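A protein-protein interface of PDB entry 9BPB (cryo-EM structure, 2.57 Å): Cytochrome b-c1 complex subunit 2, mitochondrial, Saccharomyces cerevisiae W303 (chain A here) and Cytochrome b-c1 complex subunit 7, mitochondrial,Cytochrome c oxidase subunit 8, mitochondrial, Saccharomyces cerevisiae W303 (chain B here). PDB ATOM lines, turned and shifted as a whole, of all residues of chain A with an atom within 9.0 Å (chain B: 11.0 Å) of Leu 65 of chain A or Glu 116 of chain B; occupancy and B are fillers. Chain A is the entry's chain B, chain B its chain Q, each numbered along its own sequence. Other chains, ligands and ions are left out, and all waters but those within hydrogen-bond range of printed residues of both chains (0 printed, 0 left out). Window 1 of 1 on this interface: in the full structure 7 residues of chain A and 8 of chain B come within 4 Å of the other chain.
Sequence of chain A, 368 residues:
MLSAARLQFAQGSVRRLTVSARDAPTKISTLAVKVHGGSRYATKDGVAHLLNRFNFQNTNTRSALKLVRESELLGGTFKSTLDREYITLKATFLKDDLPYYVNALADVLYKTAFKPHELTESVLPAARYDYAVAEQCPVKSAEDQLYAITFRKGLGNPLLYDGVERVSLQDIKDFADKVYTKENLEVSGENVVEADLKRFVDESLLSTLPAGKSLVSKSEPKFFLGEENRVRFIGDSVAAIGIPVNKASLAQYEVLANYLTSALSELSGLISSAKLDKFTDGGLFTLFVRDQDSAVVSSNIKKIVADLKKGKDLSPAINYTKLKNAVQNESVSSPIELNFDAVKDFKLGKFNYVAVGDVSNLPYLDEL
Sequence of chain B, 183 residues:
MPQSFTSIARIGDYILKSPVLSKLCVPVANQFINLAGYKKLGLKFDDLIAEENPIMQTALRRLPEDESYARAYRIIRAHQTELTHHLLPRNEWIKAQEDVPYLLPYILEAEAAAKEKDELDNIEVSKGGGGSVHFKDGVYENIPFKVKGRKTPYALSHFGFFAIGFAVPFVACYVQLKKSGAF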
ATOM      1  N   PHE A  56      26.808  28.945 -13.087  1.00  0.00           N
ATOM      2  CA  PHE A  56      26.231  27.801 -12.374  1.00  0.00           C
ATOM      3  C   PHE A  56      26.622  26.468 -12.997  1.00  0.00           C
ATOM      4  O   PHE A  56      25.885  25.484 -12.849  1.00  0.00           O
ATOM      5  CB  PHE A  56      24.709  27.904 -12.253  1.00  0.00           C
ATOM      6  CG  PHE A  56      24.263  29.086 -11.453  1.00  0.00           C
ATOM      7  CD1 PHE A  56      24.505  29.142 -10.093  1.00  0.00           C
ATOM      8  CD2 PHE A  56      23.644  30.161 -12.064  1.00  0.00           C
ATOM      9  CE1 PHE A  56      24.121  30.234  -9.358  1.00  0.00           C
ATOM     10  CE2 PHE A  56      23.255  31.256 -11.331  1.00  0.00           C
ATOM     11  CZ  PHE A  56      23.491  31.290  -9.974  1.00  0.00           C
ATOM     12  N   GLN A  57      27.753  26.405 -13.694  1.00  0.00           N
ATOM     13  CA  GLN A  57      28.373  25.136 -14.041  1.00  0.00           C
ATOM     14  C   GLN A  57      29.215  24.650 -12.862  1.00  0.00           C
ATOM     15  O   GLN A  57      29.140  25.184 -11.752  1.00  0.00           O
ATOM     16  CB  GLN A  57      29.215  25.278 -15.305  1.00  0.00           C
ATOM     17  CG  GLN A  57      28.432  25.171 -16.610  1.00  0.00           C
ATOM     18  CD  GLN A  57      27.946  23.763 -16.897  1.00  0.00           C
ATOM     19  OE1 GLN A  57      28.735  22.820 -16.940  1.00  0.00           O
ATOM     20  NE2 GLN A  57      26.645  23.616 -17.110  1.00  0.00           N
ATOM     21  N   ASN A  58      30.033  23.626 -13.105  1.00  0.00           N
ATOM     22  CA  ASN A  58      30.836  23.042 -12.038  1.00  0.00           C
ATOM     23  C   ASN A  58      31.835  24.051 -11.485  1.00  0.00           C
ATOM     24  O   ASN A  58      32.405  24.859 -12.224  1.00  0.00           O
ATOM     25  CB  ASN A  58      31.583  21.806 -12.540  1.00  0.00           C
ATOM     26  CG  ASN A  58      30.671  20.630 -12.780  1.00  0.00           C
ATOM     27  OD1 ASN A  58      29.452  20.759 -12.743  1.00  0.00           O
ATOM     28  ND2 ASN A  58      31.258  19.467 -13.020  1.00  0.00           N
ATOM     29  N   THR A  59      32.039  24.000 -10.171  1.00  0.00           N
ATOM     30  CA  THR A  59      33.116  24.713  -9.504  1.00  0.00           C
ATOM     31  C   THR A  59      34.166  23.707  -9.055  1.00  0.00           C
ATOM     32  O   THR A  59      34.044  22.502  -9.293  1.00  0.00           O
ATOM     33  CB  THR A  59      32.615  25.512  -8.296  1.00  0.00           C
ATOM     34  OG1 THR A  59      31.809  24.668  -7.466  1.00  0.00           O
ATOM     35  CG2 THR A  59      31.802  26.718  -8.745  1.00  0.00           C
ATOM     36  N   ASN A  60      35.212  24.218  -8.402  1.00  0.00           N
ATOM     37  CA  ASN A  60      36.284  23.340  -7.942  1.00  0.00           C
ATOM     38  C   ASN A  60      35.805  22.400  -6.843  1.00  0.00           C
ATOM     39  O   ASN A  60      36.125  21.206  -6.855  1.00  0.00           O
ATOM     40  CB  ASN A  60      37.476  24.171  -7.465  1.00  0.00           C
ATOM     41  CG  ASN A  60      38.240  24.802  -8.610  1.00  0.00           C
ATOM     42  OD1 ASN A  60      38.217  24.304  -9.735  1.00  0.00           O
ATOM     43  ND2 ASN A  60      38.926  25.903  -8.330  1.00  0.00           N
ATOM     44  N   THR A  61      35.023  22.915  -5.891  1.00  0.00           N
ATOM     45  CA  THR A  61      34.590  22.091  -4.766  1.00  0.00           C
ATOM     46  C   THR A  61      33.375  21.245  -5.129  1.00  0.00           C
ATOM     47  O   THR A  61      33.414  20.013  -5.030  1.00  0.00           O
ATOM     48  CB  THR A  61      34.286  22.973  -3.555  1.00  0.00           C
ATOM     49  OG1 THR A  61      35.510  23.487  -3.018  1.00  0.00           O
ATOM     50  CG2 THR A  61      33.561  22.178  -2.481  1.00  0.00           C
ATOM     51  N   ARG A  62      32.288  21.883  -5.553  1.00  0.00           N
ATOM     52  CA  ARG A  62      31.031  21.193  -5.799  1.00  0.00           C
ATOM     53  C   ARG A  62      30.683  21.257  -7.279  1.00  0.00           C
ATOM     54  O   ARG A  62      30.912  22.276  -7.937  1.00  0.00           O
ATOM     55  CB  ARG A  62      29.896  21.797  -4.962  1.00  0.00           C
ATOM     56  CG  ARG A  62      29.479  23.195  -5.390  1.00  0.00           C
ATOM     57  CD  ARG A  62      28.393  23.763  -4.496  1.00  0.00           C
ATOM     58  NE  ARG A  62      28.906  24.110  -3.176  1.00  0.00           N
ATOM     59  CZ  ARG A  62      28.170  24.615  -2.196  1.00  0.00           C
ATOM     60  NH1 ARG A  62      26.881  24.859  -2.354  1.00  0.00           N
ATOM     61  NH2 ARG A  62      28.745  24.889  -1.029  1.00  0.00           N
ATOM     62  N   SER A  63      30.141  20.160  -7.797  1.00  0.00           N
ATOM     63  CA  SER A  63      29.691  20.130  -9.179  1.00  0.00           C
ATOM     64  C   SER A  63      28.349  20.843  -9.322  1.00  0.00           C
ATOM     65  O   SER A  63      27.667  21.147  -8.341  1.00  0.00           O
ATOM     66  CB  SER A  63      29.587  18.687  -9.677  1.00  0.00           C
ATOM     67  OG  SER A  63      28.431  18.045  -9.177  1.00  0.00           O
ATOM     68  N   ALA A  64      27.976  21.124 -10.572  1.00  0.00           N
ATOM     69  CA  ALA A  64      26.691  21.769 -10.822  1.00  0.00           C
ATOM     70  C   ALA A  64      25.533  20.817 -10.548  1.00  0.00           C
ATOM     71  O   ALA A  64      24.400  21.256 -10.321  1.00  0.00           O
ATOM     72  CB  ALA A  64      26.632  22.295 -12.256  1.00  0.00           C
ATOM     73  N   LEU A  65      25.792  19.508 -10.581  1.00  0.00           N
ATOM     74  CA  LEU A  65      24.788  18.545 -10.135  1.00  0.00           C
ATOM     75  C   LEU A  65      24.720  18.499  -8.612  1.00  0.00           C
ATOM     76  O   LEU A  65      23.665  18.210  -8.035  1.00  0.00           O
ATOM     77  CB  LEU A  65      25.098  17.163 -10.711  1.00  0.00           C
ATOM     78  CG  LEU A  65      24.313  15.965 -10.168  1.00  0.00           C
ATOM     79  CD1 LEU A  65      22.908  15.949 -10.719  1.00  0.00           C
ATOM     80  CD2 LEU A  65      25.027  14.669 -10.490  1.00  0.00           C
ATOM     81  N   LYS A  66      25.843  18.777  -7.948  1.00  0.00           N
ATOM     82  CA  LYS A  66      25.854  18.866  -6.492  1.00  0.00           C
ATOM     83  C   LYS A  66      25.017  20.045  -6.016  1.00  0.00           C
ATOM     84  O   LYS A  66      24.345  19.967  -4.981  1.00  0.00           O
ATOM     85  CB  LYS A  66      27.293  18.999  -5.998  1.00  0.00           C
ATOM     86  CG  LYS A  66      27.468  19.130  -4.502  1.00  0.00           C
ATOM     87  CD  LYS A  66      27.322  17.778  -3.828  1.00  0.00           C
ATOM     88  CE  LYS A  66      27.594  17.867  -2.338  1.00  0.00           C
ATOM     89  NZ  LYS A  66      29.005  18.245  -2.056  1.00  0.00           N
ATOM     90  N   LEU A  67      25.048  21.150  -6.764  1.00  0.00           N
ATOM     91  CA  LEU A  67      24.311  22.344  -6.369  1.00  0.00           C
ATOM     92  C   LEU A  67      22.806  22.136  -6.485  1.00  0.00           C
ATOM     93  O   LEU A  67      22.026  22.803  -5.797  1.00  0.00           O
ATOM     94  CB  LEU A  67      24.759  23.527  -7.225  1.00  0.00           C
ATOM     95  CG  LEU A  67      24.267  24.924  -6.847  1.00  0.00           C
ATOM     96  CD1 LEU A  67      24.775  25.329  -5.474  1.00  0.00           C
ATOM     97  CD2 LEU A  67      24.701  25.931  -7.895  1.00  0.00           C
ATOM     98  N   VAL A  68      22.379  21.217  -7.352  1.00  0.00           N
ATOM     99  CA  VAL A  68      20.950  21.043  -7.611  1.00  0.00           C
ATOM    100  C   VAL A  68      20.271  20.338  -6.445  1.00  0.00           C
ATOM    101  O   VAL A  68      19.277  20.827  -5.897  1.00  0.00           O
ATOM    102  CB  VAL A  68      20.732  20.282  -8.930  1.00  0.00           C
ATOM    103  CG1 VAL A  68      19.278  19.887  -9.073  1.00  0.00           C
ATOM    104  CG2 VAL A  68      21.154  21.144 -10.105  1.00  0.00           C
ATOM    105  N   ARG A  69      20.792  19.175  -6.051  1.00  0.00           N
ATOM    106  CA  ARG A  69      20.143  18.387  -5.006  1.00  0.00           C
ATOM    107  C   ARG A  69      20.182  19.093  -3.655  1.00  0.00           C
ATOM    108  O   ARG A  69      19.392  18.772  -2.761  1.00  0.00           O
ATOM    109  CB  ARG A  69      20.788  17.006  -4.908  1.00  0.00           C
ATOM    110  CG  ARG A  69      21.062  16.349  -6.251  1.00  0.00           C
ATOM    111  CD  ARG A  69      19.782  15.879  -6.918  1.00  0.00           C
ATOM    112  NE  ARG A  69      20.036  15.338  -8.245  1.00  0.00           N
ATOM    113  CZ  ARG A  69      19.795  14.085  -8.604  1.00  0.00           C
ATOM    114  NH1 ARG A  69      19.272  13.214  -7.759  1.00  0.00           N
ATOM    115  NH2 ARG A  69      20.084  13.696  -9.842  1.00  0.00           N
ATOM    116  N   GLU A  70      21.099  20.049  -3.478  1.00  0.00           N
ATOM    117  CA  GLU A  70      21.162  20.775  -2.214  1.00  0.00           C
ATOM    118  C   GLU A  70      20.206  21.962  -2.193  1.00  0.00           C
ATOM    119  O   GLU A  70      19.458  22.142  -1.226  1.00  0.00           O
ATOM    120  CB  GLU A  70      22.583  21.249  -1.932  1.00  0.00           C
ATOM    121  CG  GLU A  70      23.569  20.154  -1.621  1.00  0.00           C
ATOM    122  CD  GLU A  70      24.955  20.707  -1.382  1.00  0.00           C
ATOM    123  OE1 GLU A  70      25.159  21.916  -1.618  1.00  0.00           O
ATOM    124  OE2 GLU A  70      25.830  19.940  -0.934  1.00  0.00           O
ATOM    125  N   SER A  71      20.227  22.796  -3.234  1.00  0.00           N
ATOM    126  CA  SER A  71      19.366  23.973  -3.231  1.00  0.00           C
ATOM    127  C   SER A  71      17.902  23.582  -3.375  1.00  0.00           C
ATOM    128  O   SER A  71      17.009  24.396  -3.116  1.00  0.00           O
ATOM    129  CB  SER A  71      19.776  24.936  -4.343  1.00  0.00           C
ATOM    130  OG  SER A  71      19.570  24.364  -5.618  1.00  0.00           O
ATOM    131  N   GLU A  72      17.637  22.342  -3.791  1.00  0.00           N
ATOM    132  CA  GLU A  72      16.259  21.876  -3.893  1.00  0.00           C
ATOM    133  C   GLU A  72      15.653  21.636  -2.520  1.00  0.00           C
ATOM    134  O   GLU A  72      14.513  22.036  -2.258  1.00  0.00           O
ATOM    135  CB  GLU A  72      16.195  20.594  -4.721  1.00  0.00           C
ATOM    136  CG  GLU A  72      15.992  20.825  -6.201  1.00  0.00           C
ATOM    137  CD  GLU A  72      15.973  19.538  -6.984  1.00  0.00           C
ATOM    138  OE1 GLU A  72      16.165  18.470  -6.371  1.00  0.00           O
ATOM    139  OE2 GLU A  72      15.765  19.594  -8.212  1.00  0.00           O
ATOM    140  N   GLU A 118      32.924  21.309 -20.690  1.00  0.00           N
ATOM    141  CA  GLU A 118      31.680  21.989 -20.345  1.00  0.00           C
ATOM    142  C   GLU A 118      31.242  22.931 -21.457  1.00  0.00           C
ATOM    143  O   GLU A 118      30.056  23.260 -21.571  1.00  0.00           O
ATOM    144  CB  GLU A 118      31.844  22.734 -19.023  1.00  0.00           C
ATOM    145  CG  GLU A 118      32.056  21.802 -17.843  1.00  0.00           C
ATOM    146  CD  GLU A 118      32.287  22.538 -16.541  1.00  0.00           C
ATOM    147  OE1 GLU A 118      33.296  23.264 -16.438  1.00  0.00           O
ATOM    148  OE2 GLU A 118      31.456  22.389 -15.624  1.00  0.00           O
ATOM    149  N   THR B   6      39.777   4.162 -10.196  1.00  0.00           N
ATOM    150  CA  THR B   6      40.153   4.915  -9.003  1.00  0.00           C
ATOM    151  C   THR B   6      40.529   3.973  -7.871  1.00  0.00           C
ATOM    152  O   THR B   6      41.393   4.293  -7.047  1.00  0.00           O
ATOM    153  CB  THR B   6      39.010   5.831  -8.564  1.00  0.00           C
ATOM    154  OG1 THR B   6      37.878   5.033  -8.195  1.00  0.00           O
ATOM    155  CG2 THR B   6      38.615   6.775  -9.683  1.00  0.00           C
ATOM    156  N   ILE B  55      31.408   4.677 -19.442  1.00  0.00           N
ATOM    157  CA  ILE B  55      32.479   5.450 -18.819  1.00  0.00           C
ATOM    158  C   ILE B  55      33.622   5.764 -19.781  1.00  0.00           C
ATOM    159  O   ILE B  55      34.033   6.927 -19.877  1.00  0.00           O
ATOM    160  CB  ILE B  55      33.045   4.728 -17.583  1.00  0.00           C
ATOM    161  CG1 ILE B  55      31.958   4.536 -16.529  1.00  0.00           C
ATOM    162  CG2 ILE B  55      34.209   5.511 -16.995  1.00  0.00           C
ATOM    163  CD1 ILE B  55      31.492   5.831 -15.906  1.00  0.00           C
ATOM    164  N   ARG B  62      36.043  13.366 -24.844  1.00  0.00           N
ATOM    165  CA  ARG B  62      36.789  14.528 -24.377  1.00  0.00           C
ATOM    166  C   ARG B  62      38.232  14.529 -24.856  1.00  0.00           C
ATOM    167  O   ARG B  62      38.907  15.555 -24.722  1.00  0.00           O
ATOM    168  CB  ARG B  62      36.759  14.608 -22.846  1.00  0.00           C
ATOM    169  CG  ARG B  62      35.410  14.331 -22.195  1.00  0.00           C
ATOM    170  CD  ARG B  62      35.425  14.830 -20.754  1.00  0.00           C
ATOM    171  NE  ARG B  62      34.372  14.263 -19.920  1.00  0.00           N
ATOM    172  CZ  ARG B  62      33.113  14.680 -19.900  1.00  0.00           C
ATOM    173  NH1 ARG B  62      32.697  15.658 -20.682  1.00  0.00           N
ATOM    174  NH2 ARG B  62      32.251  14.099 -19.072  1.00  0.00           N
ATOM    175  N   LEU B 108      39.506   9.360 -14.878  1.00  0.00           N
ATOM    176  CA  LEU B 108      39.326   9.683 -13.466  1.00  0.00           C
ATOM    177  C   LEU B 108      38.291  10.782 -13.256  1.00  0.00           C
ATOM    178  O   LEU B 108      37.501  10.708 -12.309  1.00  0.00           O
ATOM    179  CB  LEU B 108      40.658  10.087 -12.836  1.00  0.00           C
ATOM    180  CG  LEU B 108      41.704   8.988 -12.647  1.00  0.00           C
ATOM    181  CD1 LEU B 108      42.771   9.425 -11.666  1.00  0.00           C
ATOM    182  CD2 LEU B 108      41.061   7.697 -12.191  1.00  0.00           C
ATOM    183  N   GLU B 109      38.273  11.803 -14.111  1.00  0.00           N
ATOM    184  CA  GLU B 109      37.291  12.866 -13.947  1.00  0.00           C
ATOM    185  C   GLU B 109      35.886  12.430 -14.320  1.00  0.00           C
ATOM    186  O   GLU B 109      34.929  13.150 -14.017  1.00  0.00           O
ATOM    187  CB  GLU B 109      37.657  14.092 -14.789  1.00  0.00           C
ATOM    188  CG  GLU B 109      37.378  13.932 -16.271  1.00  0.00           C
ATOM    189  CD  GLU B 109      37.707  15.179 -17.065  1.00  0.00           C
ATOM    190  OE1 GLU B 109      38.185  16.160 -16.459  1.00  0.00           O
ATOM    191  OE2 GLU B 109      37.489  15.179 -18.293  1.00  0.00           O
ATOM    192  N   ALA B 110      35.740  11.278 -14.969  1.00  0.00           N
ATOM    193  CA  ALA B 110      34.443  10.784 -15.398  1.00  0.00           C
ATOM    194  C   ALA B 110      33.820   9.829 -14.399  1.00  0.00           C
ATOM    195  O   ALA B 110      32.595   9.710 -14.361  1.00  0.00           O
ATOM    196  CB  ALA B 110      34.561  10.096 -16.759  1.00  0.00           C
ATOM    197  N   GLU B 111      34.631   9.148 -13.591  1.00  0.00           N
ATOM    198  CA  GLU B 111      34.125   8.245 -12.565  1.00  0.00           C
ATOM    199  C   GLU B 111      33.736   8.965 -11.284  1.00  0.00           C
ATOM    200  O   GLU B 111      32.777   8.564 -10.623  1.00  0.00           O
ATOM    201  CB  GLU B 111      35.157   7.162 -12.238  1.00  0.00           C
ATOM    202  CG  GLU B 111      35.289   6.079 -13.290  1.00  0.00           C
ATOM    203  CD  GLU B 111      36.099   4.898 -12.795  1.00  0.00           C
ATOM    204  OE1 GLU B 111      36.616   4.966 -11.662  1.00  0.00           O
ATOM    205  OE2 GLU B 111      36.215   3.899 -13.533  1.00  0.00           O
ATOM    206  N   ALA B 112      34.462  10.018 -10.915  1.00  0.00           N
ATOM    207  CA  ALA B 112      34.127  10.794  -9.730  1.00  0.00           C
ATOM    208  C   ALA B 112      32.882  11.647  -9.918  1.00  0.00           C
ATOM    209  O   ALA B 112      32.232  11.988  -8.925  1.00  0.00           O
ATOM    210  CB  ALA B 112      35.306  11.684  -9.330  1.00  0.00           C
ATOM    211  N   ALA B 113      32.538  12.000 -11.153  1.00  0.00           N
ATOM    212  CA  ALA B 113      31.279  12.661 -11.454  1.00  0.00           C
ATOM    213  C   ALA B 113      30.132  11.670 -11.596  1.00  0.00           C
ATOM    214  O   ALA B 113      28.969  12.053 -11.443  1.00  0.00           O
ATOM    215  CB  ALA B 113      31.412  13.505 -12.722  1.00  0.00           C
ATOM    216  N   ALA B 114      30.435  10.403 -11.879  1.00  0.00           N
ATOM    217  CA  ALA B 114      29.438   9.348 -11.885  1.00  0.00           C
ATOM    218  C   ALA B 114      29.342   8.602 -10.565  1.00  0.00           C
ATOM    219  O   ALA B 114      28.335   7.921 -10.338  1.00  0.00           O
ATOM    220  CB  ALA B 114      29.722   8.338 -13.006  1.00  0.00           C
ATOM    221  N   LYS B 115      30.357   8.688  -9.704  1.00  0.00           N
ATOM    222  CA  LYS B 115      30.195   8.231  -8.329  1.00  0.00           C
ATOM    223  C   LYS B 115      29.279   9.168  -7.559  1.00  0.00           C
ATOM    224  O   LYS B 115      28.467   8.724  -6.740  1.00  0.00           O
ATOM    225  CB  LYS B 115      31.555   8.128  -7.641  1.00  0.00           C
ATOM    226  CG  LYS B 115      31.476   7.861  -6.150  1.00  0.00           C
ATOM    227  CD  LYS B 115      32.862   7.759  -5.536  1.00  0.00           C
ATOM    228  CE  LYS B 115      32.806   7.794  -4.016  1.00  0.00           C
ATOM    229  NZ  LYS B 115      32.152   9.032  -3.508  1.00  0.00           N
ATOM    230  N   GLU B 116      29.396  10.470  -7.822  1.00  0.00           N
ATOM    231  CA  GLU B 116      28.552  11.459  -7.169  1.00  0.00           C
ATOM    232  C   GLU B 116      27.083  11.255  -7.510  1.00  0.00           C
ATOM    233  O   GLU B 116      26.221  11.414  -6.642  1.00  0.00           O
ATOM    234  CB  GLU B 116      29.021  12.857  -7.567  1.00  0.00           C
ATOM    235  CG  GLU B 116      28.134  13.995  -7.124  1.00  0.00           C
ATOM    236  CD  GLU B 116      28.333  15.232  -7.978  1.00  0.00           C
ATOM    237  OE1 GLU B 116      28.173  15.135  -9.214  1.00  0.00           O
ATOM    238  OE2 GLU B 116      28.647  16.304  -7.418  1.00  0.00           O
ATOM    239  N   LYS B 117      26.784  10.904  -8.762  1.00  0.00           N
ATOM    240  CA  LYS B 117      25.399  10.689  -9.169  1.00  0.00           C
ATOM    241  C   LYS B 117      24.744   9.554  -8.395  1.00  0.00           C
ATOM    242  O   LYS B 117      23.601   9.693  -7.953  1.00  0.00           O
ATOM    243  CB  LYS B 117      25.338  10.403 -10.670  1.00  0.00           C
ATOM    244  CG  LYS B 117      23.944  10.456 -11.268  1.00  0.00           C
ATOM    245  CD  LYS B 117      23.704  11.760 -12.002  1.00  0.00           C
ATOM    246  CE  LYS B 117      22.259  11.877 -12.457  1.00  0.00           C
ATOM    247  NZ  LYS B 117      21.775  13.280 -12.397  1.00  0.00           N
ATOM    248  N   ASP B 118      25.443   8.433  -8.218  1.00  0.00           N
ATOM    249  CA  ASP B 118      24.845   7.291  -7.533  1.00  0.00           C
ATOM    250  C   ASP B 118      24.790   7.481  -6.022  1.00  0.00           C
ATOM    251  O   ASP B 118      23.984   6.826  -5.351  1.00  0.00           O
ATOM    252  CB  ASP B 118      25.608   6.011  -7.872  1.00  0.00           C
ATOM    253  CG  ASP B 118      24.716   4.789  -7.870  1.00  0.00           C
ATOM    254  OD1 ASP B 118      23.512   4.934  -7.577  1.00  0.00           O
ATOM    255  OD2 ASP B 118      25.217   3.684  -8.164  1.00  0.00           O
ATOM    256  N   GLU B 119      25.630   8.357  -5.471  1.00  0.00           N
ATOM    257  CA  GLU B 119      25.605   8.676  -4.051  1.00  0.00           C
ATOM    258  C   GLU B 119      24.603   9.776  -3.725  1.00  0.00           C
ATOM    259  O   GLU B 119      24.310  10.012  -2.549  1.00  0.00           O
ATOM    260  CB  GLU B 119      27.005   9.074  -3.580  1.00  0.00           C
ATOM    261  CG  GLU B 119      27.231   8.945  -2.086  1.00  0.00           C
ATOM    262  CD  GLU B 119      28.636   9.330  -1.678  1.00  0.00           C
ATOM    263  OE1 GLU B 119      29.398   9.798  -2.550  1.00  0.00           O
ATOM    264  OE2 GLU B 119      28.980   9.167  -0.489  1.00  0.00           O
ATOM    265  N   LEU B 120      24.068  10.449  -4.745  1.00  0.00           N
ATOM    266  CA  LEU B 120      23.003  11.419  -4.567  1.00  0.00           C
ATOM    267  C   LEU B 120      21.620  10.847  -4.841  1.00  0.00           C
ATOM    268  O   LEU B 120      20.633  11.425  -4.378  1.00  0.00           O
ATOM    269  CB  LEU B 120      23.222  12.636  -5.478  1.00  0.00           C
ATOM    270  CG  LEU B 120      24.287  13.638  -5.039  1.00  0.00           C
ATOM    271  CD1 LEU B 120      24.361  14.806  -6.008  1.00  0.00           C
ATOM    272  CD2 LEU B 120      24.006  14.126  -3.630  1.00  0.00           C
ATOM    273  N   ASP B 121      21.519   9.743  -5.572  1.00  0.00           N
ATOM    274  CA  ASP B 121      20.248   9.076  -5.809  1.00  0.00           C
ATOM    275  C   ASP B 121      19.766   8.286  -4.605  1.00  0.00           C
ATOM    276  O   ASP B 121      18.635   7.790  -4.622  1.00  0.00           O
ATOM    277  CB  ASP B 121      20.361   8.144  -7.017  1.00  0.00           C
ATOM    278  CG  ASP B 121      20.532   8.898  -8.321  1.00  0.00           C
ATOM    279  OD1 ASP B 121      20.838  10.106  -8.274  1.00  0.00           O
ATOM    280  OD2 ASP B 121      20.363   8.281  -9.392  1.00  0.00           O
ATOM    281  N   ASN B 122      20.590   8.150  -3.571  1.00  0.00           N
ATOM    282  CA  ASN B 122      20.245   7.370  -2.387  1.00  0.00           C
ATOM    283  C   ASN B 122      20.598   8.143  -1.123  1.00  0.00           C
ATOM    284  O   ASN B 122      21.211   7.615  -0.194  1.00  0.00           O
ATOM    285  CB  ASN B 122      20.941   6.010  -2.405  1.00  0.00           C
ATOM    286  CG  ASN B 122      20.380   5.081  -3.461  1.00  0.00           C
ATOM    287  OD1 ASN B 122      19.169   4.902  -3.565  1.00  0.00           O
ATOM    288  ND2 ASN B 122      21.262   4.481  -4.250  1.00  0.00           N
ATOM    289  N   ILE B 123      20.214   9.413  -1.069  1.00  0.00           N
ATOM    290  CA  ILE B 123      20.436  10.244   0.109  1.00  0.00           C
ATOM    291  C   ILE B 123      19.239  10.105   1.038  1.00  0.00           C
ATOM    292  O   ILE B 123      18.090  10.294   0.621  1.00  0.00           O
ATOM    293  CB  ILE B 123      20.683  11.714  -0.272  1.00  0.00           C
ATOM    294  CG1 ILE B 123      19.620  12.219  -1.248  1.00  0.00           C
ATOM    295  CG2 ILE B 123      22.077  11.890  -0.850  1.00  0.00           C
ATOM    296  CD1 ILE B 123      19.704  13.708  -1.519  1.00  0.00           C
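OG of Ser 63 of chain A sits at hydrogen-bond distance from OE2 of Glu 116 of chain B (2.5 Å).
NH1 of Arg 69 of chain A lies within salt-bridge range of OD1 of Asp 121 of chain B, 3.5 Å away.
NH2 of Arg 69 of chain A lies close to NZ of Lys 117 of chain B, 3.1 Å away.
OG of Ser 63 of chain A lies close to N of Leu 65 of chain A, at 3.3 Å.
OG of Ser 63 of chain A sits at hydrogen-bond distance from N of Lys 66 of chain A.
The side-chain carboxylate of Glu 70 of chain A is in salt-bridge range of the side-chain amino group of Lys 66 of chain A (3.8 Å).
Among the printed residues, pairs that only touch across the chains: Lys 66 of chain A with Glu 116 of chain B (3.3 Å), Leu 65 of chain A with Lys 117 of chain B (3.4 Å), Leu 65 of chain A with Glu 116 of chain B (3.4 Å) and Arg 69 of chain A with Leu 120 of chain B (3.7 Å).
Ser 63 of chain A touches just one residue of chain B: Glu 116 (2.5 Å).
Lys 66 of chain A touches just one residue of chain B: Glu 116 (3.3 Å).
Of the printed residues of chain A, Leu 120 of chain B touches Arg 69 (3.7 Å).
Of the printed residues of chain A, Asp 121 of chain B touches Arg 69 (3.5 Å).
The nearest printed residue of chain A that does not touch Asp 121 of chain B is Leu 65 of chain A (6.6 Å).
Of the 19 printed residues of chain B, 4 touch a printed residue of chain A.
Printed residues of chain B that touch a printed residue of chain A: Glu 116, Lys 117, Leu 120 and Asp 121.
Of the 18 printed residues of chain A, 4 touch a printed residue of chain B.
Hydrophobic or aromatic side chains of chain A that line the printed part of chain B: Leu 65.
Among the printed residues, 7 pairs touch across the chains.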
